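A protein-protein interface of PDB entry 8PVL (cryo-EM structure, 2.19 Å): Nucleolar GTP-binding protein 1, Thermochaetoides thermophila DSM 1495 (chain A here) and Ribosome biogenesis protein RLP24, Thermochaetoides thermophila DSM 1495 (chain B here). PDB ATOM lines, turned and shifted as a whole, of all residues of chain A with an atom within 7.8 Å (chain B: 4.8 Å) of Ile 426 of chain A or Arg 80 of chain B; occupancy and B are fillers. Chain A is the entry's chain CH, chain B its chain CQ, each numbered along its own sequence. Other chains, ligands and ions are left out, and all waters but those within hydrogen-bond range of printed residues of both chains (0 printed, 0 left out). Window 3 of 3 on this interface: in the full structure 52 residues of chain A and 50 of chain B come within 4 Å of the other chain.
The indole nitrogen of Trp 432 of chain A sits close to the side-chain amide nitrogen of Asn 429 of chain A.
Among the printed residues, pairs that only touch across the chains: Leu 427 of chain A with Tyr 81 of chain B (3.9 Å), Trp 432 of chain A with Tyr 81 of chain B (3.6 Å), Trp 432 of chain A with Asn 82 of chain B (3.4 Å) and Ile 450 of chain A with Trp 86 of chain B (3.5 Å).
Ile 426 of chain A touches just one residue of chain B: Arg 80 (2.6 Å). Asn 429 of chain A touches none of the printed residues of chain B. Of chain A, only Ile 426 comes within 4 Å of Arg 80 of chain B. Of the printed residues of chain A, Asn 82 of chain B touches Glu 428 and Trp 432. Of the printed residues of chain A, Trp 86 of chain B touches Ile 450 (3.5 Å). The nearest printed residue of chain B that does not touch Ile 426 of chain A is Tyr 81 of chain B (6.5 Å). The nearest printed residue of chain B that does not touch Ile 450 of chain A is Val 79 of chain B (4.2 Å).
NH1 of Arg 80 of chain B sits at hydrogen-bond distance from O of Ile 426 of chain A (2.6 Å). OE2 of Glu 428 of chain A lies within hydrogen-bond range of ND2 of Asn 82 of chain B (3.2 Å). The side-chain carboxylate (OE1) of Glu 428 of chain A lies close to the backbone carbonyl oxygen (O) of Tyr 81 of chain B (3.1 Å).
Printed residues of chain B that touch a printed residue of chain A: Arg 80, Tyr 81, Asn 82 and Trp 86. Hydrophobic or aromatic side chains of chain B that line the printed part of chain A: Tyr 81 and Trp 86. Of the 12 printed residues of chain A, 5 touch a printed residue of chain B. Hydrophobic or aromatic side chains of chain A within 4 Å of the printed part of chain B: Ile 426, Leu 427, Trp 432 and Ile 450. Among the printed residues, 7 pairs touch across the chains. Among the printed residues, no Asp or Glu carboxylate lies within 4 Å of a Lys or Arg side-chain nitrogen of the other chain.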
ATOM      1  N   ARG A 422     -21.934   1.273  -9.332  1.00  0.00           N
ATOM      2  CA  ARG A 422     -21.253  -0.007  -9.458  1.00  0.00           C
ATOM      3  C   ARG A 422     -21.908  -1.116  -8.650  1.00  0.00           C
ATOM      4  O   ARG A 422     -21.358  -2.219  -8.587  1.00  0.00           O
ATOM      5  CB  ARG A 422     -19.789   0.134  -9.035  1.00  0.00           C
ATOM      6  CG  ARG A 422     -18.891   0.710 -10.108  1.00  0.00           C
ATOM      7  CD  ARG A 422     -17.742   1.473  -9.495  1.00  0.00           C
ATOM      8  NE  ARG A 422     -16.782   1.919 -10.497  1.00  0.00           N
ATOM      9  CZ  ARG A 422     -15.558   1.431 -10.626  1.00  0.00           C
ATOM     10  NH1 ARG A 422     -15.119   0.452  -9.852  1.00  0.00           N
ATOM     11  NH2 ARG A 422     -14.755   1.934 -11.557  1.00  0.00           N
ATOM     12  N   LYS A 423     -23.061  -0.852  -8.029  1.00  0.00           N
ATOM     13  CA  LYS A 423     -23.705  -1.847  -7.178  1.00  0.00           C
ATOM     14  C   LYS A 423     -24.217  -3.037  -7.979  1.00  0.00           C
ATOM     15  O   LYS A 423     -24.159  -4.176  -7.501  1.00  0.00           O
ATOM     16  CB  LYS A 423     -24.851  -1.200  -6.398  1.00  0.00           C
ATOM     17  CG  LYS A 423     -25.548  -2.123  -5.413  1.00  0.00           C
ATOM     18  CD  LYS A 423     -26.578  -1.379  -4.584  1.00  0.00           C
ATOM     19  CE  LYS A 423     -27.887  -1.231  -5.343  1.00  0.00           C
ATOM     20  NZ  LYS A 423     -28.105   0.164  -5.810  1.00  0.00           N
ATOM     21  N   ASP A 424     -24.700  -2.803  -9.198  1.00  0.00           N
ATOM     22  CA  ASP A 424     -25.300  -3.845 -10.017  1.00  0.00           C
ATOM     23  C   ASP A 424     -24.363  -4.353 -11.108  1.00  0.00           C
ATOM     24  O   ASP A 424     -24.831  -4.916 -12.104  1.00  0.00           O
ATOM     25  CB  ASP A 424     -26.604  -3.338 -10.632  1.00  0.00           C
ATOM     26  CG  ASP A 424     -27.655  -3.021  -9.588  1.00  0.00           C
ATOM     27  OD1 ASP A 424     -27.492  -3.458  -8.430  1.00  0.00           O
ATOM     28  OD2 ASP A 424     -28.639  -2.331  -9.921  1.00  0.00           O
ATOM     29  N   TRP A 425     -23.056  -4.164 -10.948  1.00  0.00           N
ATOM     30  CA  TRP A 425     -22.099  -4.715 -11.896  1.00  0.00           C
ATOM     31  C   TRP A 425     -22.025  -6.229 -11.744  1.00  0.00           C
ATOM     32  O   TRP A 425     -21.958  -6.748 -10.626  1.00  0.00           O
ATOM     33  CB  TRP A 425     -20.718  -4.098 -11.686  1.00  0.00           C
ATOM     34  CG  TRP A 425     -20.512  -2.809 -12.407  1.00  0.00           C
ATOM     35  CD1 TRP A 425     -21.461  -2.062 -13.037  1.00  0.00           C
ATOM     36  CD2 TRP A 425     -19.273  -2.109 -12.574  1.00  0.00           C
ATOM     37  NE1 TRP A 425     -20.891  -0.941 -13.588  1.00  0.00           N
ATOM     38  CE2 TRP A 425     -19.549  -0.947 -13.318  1.00  0.00           C
ATOM     39  CE3 TRP A 425     -17.957  -2.355 -12.170  1.00  0.00           C
ATOM     40  CZ2 TRP A 425     -18.560  -0.029 -13.664  1.00  0.00           C
ATOM     41  CZ3 TRP A 425     -16.976  -1.442 -12.513  1.00  0.00           C
ATOM     42  CH2 TRP A 425     -17.283  -0.295 -13.254  1.00  0.00           C
ATOM     43  N   ILE A 426     -22.042  -6.938 -12.867  1.00  0.00           N
ATOM     44  CA  ILE A 426     -21.932  -8.390 -12.884  1.00  0.00           C
ATOM     45  C   ILE A 426     -20.532  -8.722 -13.384  1.00  0.00           C
ATOM     46  O   ILE A 426     -20.298  -8.820 -14.590  1.00  0.00           O
ATOM     47  CB  ILE A 426     -23.010  -9.036 -13.758  1.00  0.00           C
ATOM     48  CG1 ILE A 426     -24.317  -8.248 -13.681  1.00  0.00           C
ATOM     49  CG2 ILE A 426     -23.231 -10.482 -13.346  1.00  0.00           C
ATOM     50  CD1 ILE A 426     -25.253  -8.521 -14.837  1.00  0.00           C
ATOM     51  N   LEU A 427     -19.598  -8.899 -12.459  1.00  0.00           N
ATOM     52  CA  LEU A 427     -18.224  -9.245 -12.789  1.00  0.00           C
ATOM     53  C   LEU A 427     -17.956 -10.702 -12.445  1.00  0.00           C
ATOM     54  O   LEU A 427     -18.757 -11.373 -11.789  1.00  0.00           O
ATOM     55  CB  LEU A 427     -17.236  -8.332 -12.055  1.00  0.00           C
ATOM     56  CG  LEU A 427     -17.399  -6.826 -12.256  1.00  0.00           C
ATOM     57  CD1 LEU A 427     -16.315  -6.072 -11.511  1.00  0.00           C
ATOM     58  CD2 LEU A 427     -17.380  -6.471 -13.730  1.00  0.00           C
ATOM     59  N   GLU A 428     -16.805 -11.192 -12.911  1.00  0.00           N
ATOM     60  CA  GLU A 428     -16.408 -12.565 -12.622  1.00  0.00           C
ATOM     61  C   GLU A 428     -16.054 -12.749 -11.152  1.00  0.00           C
ATOM     62  O   GLU A 428     -16.249 -13.837 -10.600  1.00  0.00           O
ATOM     63  CB  GLU A 428     -15.233 -12.965 -13.514  1.00  0.00           C
ATOM     64  CG  GLU A 428     -15.513 -12.839 -15.010  1.00  0.00           C
ATOM     65  CD  GLU A 428     -15.075 -11.500 -15.592  1.00  0.00           C
ATOM     66  OE1 GLU A 428     -15.195 -10.471 -14.893  1.00  0.00           O
ATOM     67  OE2 GLU A 428     -14.615 -11.478 -16.753  1.00  0.00           O
ATOM     68  N   ASN A 429     -15.530 -11.709 -10.508  1.00  0.00           N
ATOM     69  CA  ASN A 429     -15.232 -11.725  -9.082  1.00  0.00           C
ATOM     70  C   ASN A 429     -15.885 -10.506  -8.445  1.00  0.00           C
ATOM     71  O   ASN A 429     -15.594  -9.371  -8.858  1.00  0.00           O
ATOM     72  CB  ASN A 429     -13.720 -11.721  -8.842  1.00  0.00           C
ATOM     73  CG  ASN A 429     -13.351 -11.987  -7.394  1.00  0.00           C
ATOM     74  OD1 ASN A 429     -14.200 -12.327  -6.572  1.00  0.00           O
ATOM     75  ND2 ASN A 429     -12.071 -11.838  -7.077  1.00  0.00           N
ATOM     76  N   PRO A 430     -16.779 -10.679  -7.463  1.00  0.00           N
ATOM     77  CA  PRO A 430     -17.427  -9.512  -6.839  1.00  0.00           C
ATOM     78  C   PRO A 430     -16.481  -8.604  -6.067  1.00  0.00           C
ATOM     79  O   PRO A 430     -16.858  -7.463  -5.774  1.00  0.00           O
ATOM     80  CB  PRO A 430     -18.469 -10.145  -5.907  1.00  0.00           C
ATOM     81  CG  PRO A 430     -18.716 -11.497  -6.481  1.00  0.00           C
ATOM     82  CD  PRO A 430     -17.401 -11.944  -7.039  1.00  0.00           C
ATOM     83  N   TRP A 432     -13.875  -7.263  -7.260  1.00  0.00           N
ATOM     84  CA  TRP A 432     -13.355  -6.286  -8.207  1.00  0.00           C
ATOM     85  C   TRP A 432     -14.315  -5.135  -8.473  1.00  0.00           C
ATOM     86  O   TRP A 432     -13.972  -4.241  -9.253  1.00  0.00           O
ATOM     87  CB  TRP A 432     -13.028  -6.958  -9.543  1.00  0.00           C
ATOM     88  CG  TRP A 432     -12.052  -8.087  -9.470  1.00  0.00           C
ATOM     89  CD1 TRP A 432     -11.151  -8.339  -8.478  1.00  0.00           C
ATOM     90  CD2 TRP A 432     -11.876  -9.121 -10.443  1.00  0.00           C
ATOM     91  NE1 TRP A 432     -10.428  -9.467  -8.771  1.00  0.00           N
ATOM     92  CE2 TRP A 432     -10.852  -9.965  -9.975  1.00  0.00           C
ATOM     93  CE3 TRP A 432     -12.485  -9.413 -11.667  1.00  0.00           C
ATOM     94  CZ2 TRP A 432     -10.425 -11.083 -10.686  1.00  0.00           C
ATOM     95  CZ3 TRP A 432     -12.060 -10.523 -12.370  1.00  0.00           C
ATOM     96  CH2 TRP A 432     -11.040 -11.344 -11.879  1.00  0.00           C
ATOM     97  N   LYS A 433     -15.501  -5.139  -7.857  1.00  0.00           N
ATOM     98  CA  LYS A 433     -16.572  -4.234  -8.259  1.00  0.00           C
ATOM     99  C   LYS A 433     -16.275  -2.772  -7.951  1.00  0.00           C
ATOM    100  O   LYS A 433     -16.852  -1.892  -8.597  1.00  0.00           O
ATOM    101  CB  LYS A 433     -17.885  -4.649  -7.590  1.00  0.00           C
ATOM    102  CG  LYS A 433     -18.966  -5.041  -8.581  1.00  0.00           C
ATOM    103  CD  LYS A 433     -20.111  -5.791  -7.922  1.00  0.00           C
ATOM    104  CE  LYS A 433     -20.741  -4.983  -6.806  1.00  0.00           C
ATOM    105  NZ  LYS A 433     -22.041  -5.567  -6.380  1.00  0.00           N
ATOM    106  N   ILE A 450      -6.706  -2.873 -24.459  1.00  0.00           N
ATOM    107  CA  ILE A 450      -7.503  -3.955 -23.884  1.00  0.00           C
ATOM    108  C   ILE A 450      -7.952  -4.894 -24.995  1.00  0.00           C
ATOM    109  O   ILE A 450      -8.598  -4.477 -25.964  1.00  0.00           O
ATOM    110  CB  ILE A 450      -8.695  -3.394 -23.100  1.00  0.00           C
ATOM    111  CG1 ILE A 450      -8.225  -2.814 -21.767  1.00  0.00           C
ATOM    112  CG2 ILE A 450      -9.738  -4.473 -22.853  1.00  0.00           C
ATOM    113  CD1 ILE A 450      -7.572  -3.829 -20.865  1.00  0.00           C
ATOM    114  N   PRO B  78     -16.964  -3.639 -26.301  1.00  0.00           N
ATOM    115  CA  PRO B  78     -16.358  -3.583 -24.968  1.00  0.00           C
ATOM    116  C   PRO B  78     -16.174  -4.963 -24.353  1.00  0.00           C
ATOM    117  O   PRO B  78     -16.852  -5.933 -24.697  1.00  0.00           O
ATOM    118  CB  PRO B  78     -17.359  -2.750 -24.161  1.00  0.00           C
ATOM    119  CG  PRO B  78     -18.656  -2.969 -24.851  1.00  0.00           C
ATOM    120  CD  PRO B  78     -18.328  -3.087 -26.311  1.00  0.00           C
ATOM    121  N   VAL B  79     -15.231  -5.027 -23.420  1.00  0.00           N
ATOM    122  CA  VAL B  79     -14.906  -6.240 -22.682  1.00  0.00           C
ATOM    123  C   VAL B  79     -15.293  -6.022 -21.227  1.00  0.00           C
ATOM    124  O   VAL B  79     -15.081  -4.934 -20.679  1.00  0.00           O
ATOM    125  CB  VAL B  79     -13.409  -6.590 -22.820  1.00  0.00           C
ATOM    126  CG1 VAL B  79     -13.065  -7.868 -22.069  1.00  0.00           C
ATOM    127  CG2 VAL B  79     -13.029  -6.718 -24.284  1.00  0.00           C
ATOM    128  N   ARG B  80     -15.903  -7.040 -20.620  1.00  0.00           N
ATOM    129  CA  ARG B  80     -16.226  -7.000 -19.199  1.00  0.00           C
ATOM    130  C   ARG B  80     -14.954  -6.842 -18.373  1.00  0.00           C
ATOM    131  O   ARG B  80     -13.923  -7.446 -18.678  1.00  0.00           O
ATOM    132  CB  ARG B  80     -16.969  -8.275 -18.802  1.00  0.00           C
ATOM    133  CG  ARG B  80     -17.504  -8.294 -17.385  1.00  0.00           C
ATOM    134  CD  ARG B  80     -18.393  -9.506 -17.170  1.00  0.00           C
ATOM    135  NE  ARG B  80     -19.427  -9.598 -18.193  1.00  0.00           N
ATOM    136  CZ  ARG B  80     -20.621  -9.031 -18.105  1.00  0.00           C
ATOM    137  NH1 ARG B  80     -20.976  -8.328 -17.042  1.00  0.00           N
ATOM    138  NH2 ARG B  80     -21.481  -9.170 -19.109  1.00  0.00           N
ATOM    139  N   TYR B  81     -15.029  -6.007 -17.335  1.00  0.00           N
ATOM    140  CA  TYR B  81     -13.842  -5.627 -16.579  1.00  0.00           C
ATOM    141  C   TYR B  81     -13.243  -6.817 -15.839  1.00  0.00           C
ATOM    142  O   TYR B  81     -13.954  -7.598 -15.200  1.00  0.00           O
ATOM    143  CB  TYR B  81     -14.167  -4.516 -15.582  1.00  0.00           C
ATOM    144  CG  TYR B  81     -13.037  -4.251 -14.612  1.00  0.00           C
ATOM    145  CD1 TYR B  81     -11.832  -3.718 -15.053  1.00  0.00           C
ATOM    146  CD2 TYR B  81     -13.166  -4.551 -13.262  1.00  0.00           C
ATOM    147  CE1 TYR B  81     -10.792  -3.485 -14.178  1.00  0.00           C
ATOM    148  CE2 TYR B  81     -12.129  -4.321 -12.379  1.00  0.00           C
ATOM    149  CZ  TYR B  81     -10.944  -3.788 -12.844  1.00  0.00           C
ATOM    150  OH  TYR B  81      -9.910  -3.553 -11.972  1.00  0.00           O
ATOM    151  N   ASN B  82     -11.921  -6.944 -15.928  1.00  0.00           N
ATOM    152  CA  ASN B  82     -11.196  -8.056 -15.325  1.00  0.00           C
ATOM    153  C   ASN B  82      -9.855  -7.528 -14.837  1.00  0.00           C
ATOM    154  O   ASN B  82      -9.058  -7.030 -15.640  1.00  0.00           O
ATOM    155  CB  ASN B  82     -11.012  -9.191 -16.336  1.00  0.00           C
ATOM    156  CG  ASN B  82     -10.691 -10.515 -15.678  1.00  0.00           C
ATOM    157  OD1 ASN B  82      -9.700 -10.646 -14.964  1.00  0.00           O
ATOM    158  ND2 ASN B  82     -11.532 -11.511 -15.923  1.00  0.00           N
ATOM    159  N   TRP B  86      -6.512  -6.386 -16.954  1.00  0.00           N
ATOM    160  CA  TRP B  86      -6.026  -5.010 -16.980  1.00  0.00           C
ATOM    161  C   TRP B  86      -4.564  -4.916 -16.546  1.00  0.00           C
ATOM    162  O   TRP B  86      -3.777  -4.174 -17.154  1.00  0.00           O
ATOM    163  CB  TRP B  86      -6.917  -4.131 -16.103  1.00  0.00           C
ATOM    164  CG  TRP B  86      -7.842  -3.259 -16.896  1.00  0.00           C
ATOM    165  CD1 TRP B  86      -7.745  -1.912 -17.068  1.00  0.00           C
ATOM    166  CD2 TRP B  86      -8.999  -3.675 -17.633  1.00  0.00           C
ATOM    167  NE1 TRP B  86      -8.770  -1.461 -17.863  1.00  0.00           N
ATOM    168  CE2 TRP B  86      -9.554  -2.524 -18.222  1.00  0.00           C
ATOM    169  CE3 TRP B  86      -9.617  -4.908 -17.854  1.00  0.00           C
ATOM    170  CZ2 TRP B  86     -10.697  -2.570 -19.014  1.00  0.00           C
ATOM    171  CZ3 TRP B  86     -10.753  -4.952 -18.638  1.00  0.00           C
ATOM    172  CH2 TRP B  86     -11.281  -3.791 -19.209  1.00  0.00           C
